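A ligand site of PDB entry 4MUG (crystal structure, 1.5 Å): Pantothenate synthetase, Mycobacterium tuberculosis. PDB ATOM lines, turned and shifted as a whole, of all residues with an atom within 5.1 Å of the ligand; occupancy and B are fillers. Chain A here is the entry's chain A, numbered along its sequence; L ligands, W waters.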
ATOM      1  N   PRO A  38      28.311   5.042 -28.543  1.00  0.00           N
ATOM      2  CA  PRO A  38      28.147   5.109 -27.093  1.00  0.00           C
ATOM      3  C   PRO A  38      26.711   5.254 -26.697  1.00  0.00           C
ATOM      4  O   PRO A  38      25.911   6.060 -27.255  1.00  0.00           O
ATOM      5  CB  PRO A  38      28.869   6.391 -26.707  1.00  0.00           C
ATOM      6  CG  PRO A  38      29.479   6.986 -28.001  1.00  0.00           C
ATOM      7  CD  PRO A  38      28.778   6.342 -29.129  1.00  0.00           C
ATOM      8  N   THR A  39      26.307   4.488 -25.728  1.00  0.00           N
ATOM      9  CA  THR A  39      24.889   4.422 -25.320  1.00  0.00           C
ATOM     10  C   THR A  39      24.813   4.397 -23.796  1.00  0.00           C
ATOM     11  O   THR A  39      25.780   3.957 -23.091  1.00  0.00           O
ATOM     12  CB  THR A  39      24.108   3.197 -25.851  1.00  0.00           C
ATOM     13  OG1 THR A  39      24.427   2.091 -24.995  1.00  0.00           O
ATOM     14  CG2 THR A  39      24.549   2.839 -27.320  1.00  0.00           C
ATOM     15  N   MET A  40      23.598   4.651 -23.304  1.00  0.00           N
ATOM     16  CA  MET A  40      23.327   4.423 -21.852  1.00  0.00           C
ATOM     17  C   MET A  40      22.411   3.208 -21.702  1.00  0.00           C
ATOM     18  O   MET A  40      21.652   3.117 -20.720  1.00  0.00           O
ATOM     19  CB  MET A  40      22.660   5.712 -21.350  1.00  0.00           C
ATOM     20  CG  MET A  40      23.698   6.795 -21.315  1.00  0.00           C
ATOM     21  SD  MET A  40      23.611   8.054 -20.000  1.00  0.00           S
ATOM     22  CE  MET A  40      22.001   8.657 -20.489  1.00  0.00           C
ATOM     23  N   HIS A  44      17.017   0.617 -28.214  1.00  0.00           N
ATOM     24  CA  HIS A  44      15.905   0.602 -29.109  1.00  0.00           C
ATOM     25  C   HIS A  44      16.371   0.647 -30.590  1.00  0.00           C
ATOM     26  O   HIS A  44      17.583   0.623 -30.895  1.00  0.00           O
ATOM     27  CB  HIS A  44      14.930   1.770 -28.770  1.00  0.00           C
ATOM     28  CG  HIS A  44      15.563   3.130 -28.856  1.00  0.00           C
ATOM     29  ND1 HIS A  44      15.727   3.979 -27.784  1.00  0.00           N
ATOM     30  CD2 HIS A  44      16.121   3.712 -29.927  1.00  0.00           C
ATOM     31  CE1 HIS A  44      16.381   5.064 -28.214  1.00  0.00           C
ATOM     32  NE2 HIS A  44      16.687   4.891 -29.487  1.00  0.00           N
ATOM     33  N   GLY A  46      16.402   2.923 -32.674  1.00  0.00           N
ATOM     34  CA  GLY A  46      17.337   4.021 -33.006  1.00  0.00           C
ATOM     35  C   GLY A  46      18.792   3.719 -32.724  1.00  0.00           C
ATOM     36  O   GLY A  46      19.687   3.973 -33.556  1.00  0.00           O
ATOM     37  N   HIS A  47      19.086   3.167 -31.554  1.00  0.00           N
ATOM     38  CA  HIS A  47      20.454   2.626 -31.323  1.00  0.00           C
ATOM     39  C   HIS A  47      20.902   1.591 -32.407  1.00  0.00           C
ATOM     40  O   HIS A  47      22.066   1.530 -32.803  1.00  0.00           O
ATOM     41  CB  HIS A  47      20.589   1.979 -29.955  1.00  0.00           C
ATOM     42  CG  HIS A  47      20.267   2.891 -28.805  1.00  0.00           C
ATOM     43  ND1 HIS A  47      19.103   2.801 -28.068  1.00  0.00           N
ATOM     44  CD2 HIS A  47      20.978   3.869 -28.228  1.00  0.00           C
ATOM     45  CE1 HIS A  47      19.089   3.716 -27.118  1.00  0.00           C
ATOM     46  NE2 HIS A  47      20.237   4.378 -27.194  1.00  0.00           N
ATOM     47  N   ALA A  49      19.981   1.489 -35.465  1.00  0.00           N
ATOM     48  CA  ALA A  49      20.365   2.229 -36.697  1.00  0.00           C
ATOM     49  C   ALA A  49      21.792   2.759 -36.519  1.00  0.00           C
ATOM     50  O   ALA A  49      22.533   2.827 -37.523  1.00  0.00           O
ATOM     51  CB  ALA A  49      19.426   3.446 -36.929  1.00  0.00           C
ATOM     52  N   LEU A  50      22.191   3.187 -35.311  1.00  0.00           N
ATOM     53  CA  LEU A  50      23.573   3.629 -35.137  1.00  0.00           C
ATOM     54  C   LEU A  50      24.543   2.480 -35.415  1.00  0.00           C
ATOM     55  O   LEU A  50      25.551   2.629 -36.082  1.00  0.00           O
ATOM     56  CB  LEU A  50      23.856   4.265 -33.755  1.00  0.00           C
ATOM     57  CG  LEU A  50      22.904   5.303 -33.258  1.00  0.00           C
ATOM     58  CD1 LEU A  50      23.385   5.840 -31.943  1.00  0.00           C
ATOM     59  CD2 LEU A  50      22.767   6.477 -34.277  1.00  0.00           C
ATOM     60  N   GLN A  72      26.147  12.954 -15.502  1.00  0.00           N
ATOM     61  CA  GLN A  72      25.239  13.809 -16.268  1.00  0.00           C
ATOM     62  C   GLN A  72      23.824  13.868 -15.630  1.00  0.00           C
ATOM     63  O   GLN A  72      22.928  14.543 -16.195  1.00  0.00           O
ATOM     64  CB  GLN A  72      25.085  13.357 -17.695  1.00  0.00           C
ATOM     65  CG  GLN A  72      24.460  11.964 -17.916  1.00  0.00           C
ATOM     66  CD  GLN A  72      24.709  11.584 -19.373  1.00  0.00           C
ATOM     67  OE1 GLN A  72      25.908  11.290 -19.789  1.00  0.00           O
ATOM     68  NE2 GLN A  72      23.644  11.674 -20.195  1.00  0.00           N
ATOM     69  N   TYR A  82      16.589   5.822 -14.303  1.00  0.00           N
ATOM     70  CA  TYR A  82      16.921   5.466 -15.689  1.00  0.00           C
ATOM     71  C   TYR A  82      16.714   3.950 -16.026  1.00  0.00           C
ATOM     72  O   TYR A  82      17.171   3.068 -15.256  1.00  0.00           O
ATOM     73  CB  TYR A  82      18.391   5.896 -16.004  1.00  0.00           C
ATOM     74  CG  TYR A  82      18.513   6.128 -17.548  1.00  0.00           C
ATOM     75  CD1 TYR A  82      17.996   7.290 -18.106  1.00  0.00           C
ATOM     76  CD2 TYR A  82      19.097   5.195 -18.392  1.00  0.00           C
ATOM     77  CE1 TYR A  82      18.025   7.502 -19.480  1.00  0.00           C
ATOM     78  CE2 TYR A  82      19.180   5.428 -19.766  1.00  0.00           C
ATOM     79  CZ  TYR A  82      18.653   6.578 -20.299  1.00  0.00           C
ATOM     80  OH  TYR A  82      18.655   6.806 -21.633  1.00  0.00           O
ATOM     81  N   HIS A 135      24.727  19.412 -16.580  1.00  0.00           N
ATOM     82  CA  HIS A 135      24.363  18.229 -17.353  1.00  0.00           C
ATOM     83  C   HIS A 135      25.373  17.953 -18.464  1.00  0.00           C
ATOM     84  O   HIS A 135      25.892  16.826 -18.669  1.00  0.00           O
ATOM     85  CB  HIS A 135      22.941  18.364 -17.958  1.00  0.00           C
ATOM     86  CG  HIS A 135      22.614  17.311 -18.964  1.00  0.00           C
ATOM     87  ND1 HIS A 135      22.407  15.991 -18.615  1.00  0.00           N
ATOM     88  CD2 HIS A 135      22.532  17.362 -20.315  1.00  0.00           C
ATOM     89  CE1 HIS A 135      22.184  15.285 -19.709  1.00  0.00           C
ATOM     90  NE2 HIS A 135      22.225  16.100 -20.754  1.00  0.00           N
ATOM     91  N   GLY A 158      22.779   9.621 -32.470  1.00  0.00           N
ATOM     92  CA  GLY A 158      21.562  10.072 -33.121  1.00  0.00           C
ATOM     93  C   GLY A 158      21.366  11.584 -33.129  1.00  0.00           C
ATOM     94  O   GLY A 158      21.925  12.319 -32.308  1.00  0.00           O
ATOM     95  N   LYS A 160      18.449  12.945 -32.540  1.00  0.00           N
ATOM     96  CA  LYS A 160      17.335  13.361 -31.690  1.00  0.00           C
ATOM     97  C   LYS A 160      17.784  14.349 -30.560  1.00  0.00           C
ATOM     98  O   LYS A 160      17.085  15.370 -30.293  1.00  0.00           O
ATOM     99  CB  LYS A 160      16.531  12.154 -31.040  1.00  0.00           C
ATOM    100  CG  LYS A 160      15.131  12.615 -30.502  1.00  0.00           C
ATOM    101  CD  LYS A 160      14.581  11.841 -29.242  1.00  0.00           C
ATOM    102  CE  LYS A 160      15.257  12.477 -28.046  1.00  0.00           C
ATOM    103  NZ  LYS A 160      15.211  11.742 -26.744  1.00  0.00           N
ATOM    104  N   ASP A 161      18.903  14.058 -29.935  1.00  0.00           N
ATOM    105  CA  ASP A 161      19.486  14.947 -28.921  1.00  0.00           C
ATOM    106  C   ASP A 161      20.503  15.785 -29.648  1.00  0.00           C
ATOM    107  O   ASP A 161      21.691  15.639 -29.605  1.00  0.00           O
ATOM    108  CB  ASP A 161      20.095  14.081 -27.749  1.00  0.00           C
ATOM    109  CG  ASP A 161      18.974  13.429 -26.916  1.00  0.00           C
ATOM    110  OD1 ASP A 161      18.469  13.991 -25.983  1.00  0.00           O
ATOM    111  OD2 ASP A 161      18.639  12.360 -27.369  1.00  0.00           O
ATOM    112  N   GLN A 164      23.060  17.974 -27.709  1.00  0.00           N
ATOM    113  CA  GLN A 164      24.150  17.082 -27.297  1.00  0.00           C
ATOM    114  C   GLN A 164      25.147  16.848 -28.455  1.00  0.00           C
ATOM    115  O   GLN A 164      26.379  16.989 -28.292  1.00  0.00           O
ATOM    116  CB  GLN A 164      23.560  15.771 -26.800  1.00  0.00           C
ATOM    117  CG  GLN A 164      24.610  14.829 -26.374  1.00  0.00           C
ATOM    118  CD  GLN A 164      24.054  13.523 -25.755  1.00  0.00           C
ATOM    119  OE1 GLN A 164      23.628  13.496 -24.646  1.00  0.00           O
ATOM    120  NE2 GLN A 164      24.070  12.443 -26.537  1.00  0.00           N
ATOM    121  N   VAL A 184      23.363  10.478 -37.091  1.00  0.00           N
ATOM    122  CA  VAL A 184      22.455   9.621 -37.834  1.00  0.00           C
ATOM    123  C   VAL A 184      21.014  10.134 -37.601  1.00  0.00           C
ATOM    124  O   VAL A 184      20.589  10.311 -36.436  1.00  0.00           O
ATOM    125  CB  VAL A 184      22.560   8.234 -37.197  1.00  0.00           C
ATOM    126  CG1 VAL A 184      21.548   7.218 -37.822  1.00  0.00           C
ATOM    127  CG2 VAL A 184      23.988   7.690 -37.399  1.00  0.00           C
ATOM    128  N   PRO A 185      20.212  10.296 -38.669  1.00  0.00           N
ATOM    129  CA  PRO A 185      18.866  10.813 -38.506  1.00  0.00           C
ATOM    130  C   PRO A 185      18.000   9.916 -37.615  1.00  0.00           C
ATOM    131  O   PRO A 185      18.144   8.659 -37.599  1.00  0.00           O
ATOM    132  CB  PRO A 185      18.352  11.002 -39.969  1.00  0.00           C
ATOM    133  CG  PRO A 185      19.629  10.992 -40.800  1.00  0.00           C
ATOM    134  CD  PRO A 185      20.610  10.100 -40.077  1.00  0.00           C
ATOM    135  N   THR A 186      17.213  10.609 -36.833  1.00  0.00           N
ATOM    136  CA  THR A 186      16.370  10.003 -35.785  1.00  0.00           C
ATOM    137  C   THR A 186      15.449   8.944 -36.386  1.00  0.00           C
ATOM    138  O   THR A 186      14.733   9.188 -37.361  1.00  0.00           O
ATOM    139  CB  THR A 186      15.499  11.074 -35.145  1.00  0.00           C
ATOM    140  OG1 THR A 186      16.395  12.039 -34.556  1.00  0.00           O
ATOM    141  CG2 THR A 186      14.587  10.492 -34.058  1.00  0.00           C
ATOM    142  N   VAL A 187      15.507   7.764 -35.759  1.00  0.00           N
ATOM    143  CA  VAL A 187      14.520   6.727 -36.093  1.00  0.00           C
ATOM    144  C   VAL A 187      13.176   7.046 -35.416  1.00  0.00           C
ATOM    145  O   VAL A 187      13.174   7.552 -34.292  1.00  0.00           O
ATOM    146  CB  VAL A 187      15.036   5.322 -35.617  1.00  0.00           C
ATOM    147  CG1 VAL A 187      14.019   4.274 -35.976  1.00  0.00           C
ATOM    148  CG2 VAL A 187      16.290   4.937 -36.368  1.00  0.00           C
ATOM    149  N   MET A 195      12.014   7.793 -31.594  1.00  0.00           N
ATOM    150  CA  MET A 195      12.492   6.782 -30.621  1.00  0.00           C
ATOM    151  C   MET A 195      13.079   7.371 -29.389  1.00  0.00           C
ATOM    152  O   MET A 195      13.724   8.462 -29.411  1.00  0.00           O
ATOM    153  CB  MET A 195      13.482   5.770 -31.272  1.00  0.00           C
ATOM    154  CG  MET A 195      12.898   4.910 -32.374  1.00  0.00           C
ATOM    155  SD  MET A 195      11.438   3.991 -31.834  1.00  0.00           S
ATOM    156  CE  MET A 195      12.271   2.573 -31.180  1.00  0.00           C
ATOM    157  N   SER A 196      12.849   6.713 -28.248  1.00  0.00           N
ATOM    158  CA  SER A 196      13.509   7.187 -27.038  1.00  0.00           C
ATOM    159  C   SER A 196      13.380   6.096 -25.984  1.00  0.00           C
ATOM    160  O   SER A 196      12.283   5.441 -25.919  1.00  0.00           O
ATOM    161  CB  SER A 196      12.796   8.401 -26.456  1.00  0.00           C
ATOM    162  OG  SER A 196      13.396   8.791 -25.208  1.00  0.00           O
ATOM    163  N   SER A 197      14.396   5.777 -25.224  1.00  0.00           N
ATOM    164  CA  SER A 197      13.941   4.790 -24.174  1.00  0.00           C
ATOM    165  C   SER A 197      13.325   5.530 -22.897  1.00  0.00           C
ATOM    166  O   SER A 197      13.216   4.979 -21.745  1.00  0.00           O
ATOM    167  CB  SER A 197      14.780   3.460 -24.004  1.00  0.00           C
ATOM    168  OG  SER A 197      14.352   2.307 -24.871  1.00  0.00           O
ATOM    169  N   ARG A 198      12.874   6.776 -23.099  1.00  0.00           N
ATOM    170  CA  ARG A 198      11.837   7.338 -22.239  1.00  0.00           C
ATOM    171  C   ARG A 198      10.364   7.139 -22.709  1.00  0.00           C
ATOM    172  O   ARG A 198       9.424   7.400 -21.955  1.00  0.00           O
ATOM    173  CB  ARG A 198      12.116   8.787 -21.826  1.00  0.00           C
ATOM    174  CG  ARG A 198      13.268   8.870 -20.848  1.00  0.00           C
ATOM    175  CD  ARG A 198      13.544  10.311 -20.390  1.00  0.00           C
ATOM    176  NE  ARG A 198      14.430  10.339 -19.221  1.00  0.00           N
ATOM    177  CZ  ARG A 198      15.679  10.822 -19.186  1.00  0.00           C
ATOM    178  NH1 ARG A 198      16.254  11.295 -20.294  1.00  0.00           N
ATOM    179  NH2 ARG A 198      16.359  10.823 -18.034  1.00  0.00           N
HETATM  180  O1  LIG L   1      16.834   7.174 -26.482  1.00  0.00           O
HETATM  181  C1  LIG L   1      16.790   8.425 -26.528  1.00  0.00           C
HETATM  182  O2  LIG L   1      16.094   9.232 -25.918  1.00  0.00           O
HETATM  183  C2  LIG L   1      17.633   9.107 -27.567  1.00  0.00           C
HETATM  184  N1  LIG L   1      18.466   8.332 -28.504  1.00  0.00           N
HETATM  185  C3  LIG L   1      18.144   8.108 -29.833  1.00  0.00           C
HETATM  186  C4  LIG L   1      16.950   8.297 -30.502  1.00  0.00           C
HETATM  187  C5  LIG L   1      16.804   7.941 -31.801  1.00  0.00           C
HETATM  188  C6  LIG L   1      17.912   7.389 -32.534  1.00  0.00           C
HETATM  189  O3  LIG L   1      17.747   7.120 -33.878  1.00  0.00           O
HETATM  190  C7  LIG L   1      18.962   7.131 -34.676  1.00  0.00           C
HETATM  191  C8  LIG L   1      19.123   7.075 -31.774  1.00  0.00           C
HETATM  192  C9  LIG L   1      19.186   7.491 -30.466  1.00  0.00           C
HETATM  193  C10 LIG L   1      20.195   7.456 -29.519  1.00  0.00           C
HETATM  194  C11 LIG L   1      19.759   7.923 -28.306  1.00  0.00           C
HETATM  195  C12 LIG L   1      20.616   8.100 -27.191  1.00  0.00           C
HETATM  196  O4  LIG L   1      21.840   7.897 -27.295  1.00  0.00           O
HETATM  197  N2  LIG L   1      20.235   8.983 -26.193  1.00  0.00           N
HETATM  198  S1  LIG L   1      21.322   9.435 -24.989  1.00  0.00           S
HETATM  199  O5  LIG L   1      22.512  10.215 -25.573  1.00  0.00           O
HETATM  200  O6  LIG L   1      21.972   8.236 -24.278  1.00  0.00           O
HETATM  201  N3  LIG L   1      20.557  10.323 -23.857  1.00  0.00           N
HETATM  202  C13 LIG L   1      19.386   9.642 -23.285  1.00  0.00           C
HETATM  203  C14 LIG L   1      19.092  10.376 -21.994  1.00  0.00           C
HETATM  204  O7  LIG L   1      18.560  11.657 -22.473  1.00  0.00           O
HETATM  205  C15 LIG L   1      19.702  12.455 -23.024  1.00  0.00           C
HETATM  206  C16 LIG L   1      20.264  11.736 -24.261  1.00  0.00           C
HETATM  207  O   HOH W   1      16.266   8.237 -23.090  1.00  0.00           O
HETATM  208  O   HOH W   2      21.722   5.792 -25.034  1.00  0.00           O
HETATM  209  O   HOH W   3      23.786  11.416 -22.911  1.00  0.00           O
HETATM  210  O   HOH W   4      19.730  11.264 -29.691  1.00  0.00           O
HETATM  211  O   HOH W   5      16.296  12.931 -24.690  1.00  0.00           O
HETATM  212  O   HOH W   6      18.561  10.352 -32.066  1.00  0.00           O
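Merely in contact with the ligand: Met 40 (3.7 Å), His 44 (2.8 Å), Gly 46 (3.2 Å), His 47 (3.7 Å), Leu 50 (3.9 Å), Tyr 82 (3.4 Å), Asp 161 (3.4 Å), Val 184 (3.98 Å), Pro 185 (3.4 Å), Thr 186 (3.7 Å) and Met 195 (3.4 Å).
Hydrophobic or aromatic side chains that line the ligand: Met 40, His 44, His 47, Leu 50, Tyr 82 and Val 187.
17 residues have an atom within 4 Å of the ligand: Met 40, His 44, Gly 46, His 47, Leu 50, Tyr 82, Lys 160, Asp 161, Gln 164, Val 184, Pro 185, Thr 186, Val 187, Met 195, Ser 196, Ser 197 and Arg 198.
The nearest printed residue that does not touch the ligand is Gly 158 (4.1 Å).
Water W2 lies within hydrogen-bond range of O6 of the ligand (2.6 Å), N of Met 40 (2.8 Å) and NE2 of His 47 (3.0 Å).
Water W1 lies within hydrogen-bond range of O2 of the ligand (3.0 Å) and OH of Tyr 82 (3.1 Å).
Water W3 lies within hydrogen-bond range of OE1 of Gln 164 (2.7 Å), NE2 of Gln 72 (2.7 Å) and O5 of the ligand (3.2 Å).
Water W5 lies within hydrogen-bond range of the side-chain amino group of Lys 160 (2.6 Å), the side-chain carboxylate of Asp 161 (2.7 Å) and an oxygen (O7) of the ligand (3.4 Å).
The guanidinium group (NH1) of Arg 198 is in hydrogen-bond range of an oxygen (O7) of the ligand (3.2 Å).
An oxygen (O5) of the ligand sits at hydrogen-bond distance from the side-chain amide nitrogen (NE2) of Gln 164 (2.9 Å).
OG of Ser 196 lies within hydrogen-bond range of O2 of the ligand, 2.8 Å away.
N of Ser 197 is in hydrogen-bond range of O1 of the ligand (3.1 Å).
N of Val 187 lies within hydrogen-bond range of O3 of the ligand.
O2 of the ligand lies within salt-bridge range of NZ of Lys 160 (2.8 Å).
The side-chain amide nitrogen (NE2) of Gln 72 sits close to the side-chain sulfur (SD) of Met 40 (3.6 Å).
The backbone carbonyl oxygen (O) of Val 187 sits at hydrogen-bond distance from the backbone NH (N) of Met 195 (2.9 Å).
The side-chain hydroxyl (OG1) of Thr 186 lies within hydrogen-bond range of the backbone NH (N) of Lys 160 (3.0 Å).
The backbone NH (N) of Ser 197 sits at hydrogen-bond distance from a ring nitrogen (ND1) of His 44 (3.4 Å).
The side-chain carboxylate (OD2) of Asp 161 lies within salt-bridge range of the side-chain amino group (NZ) of Lys 160, 3.5 Å away.
The side-chain hydroxyl (OG) of Ser 196 lies within hydrogen-bond range of the backbone NH (N) of Arg 198 (3.0 Å).
ND1 of His 47 lies within hydrogen-bond range of N of His 44 (3.0 Å).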
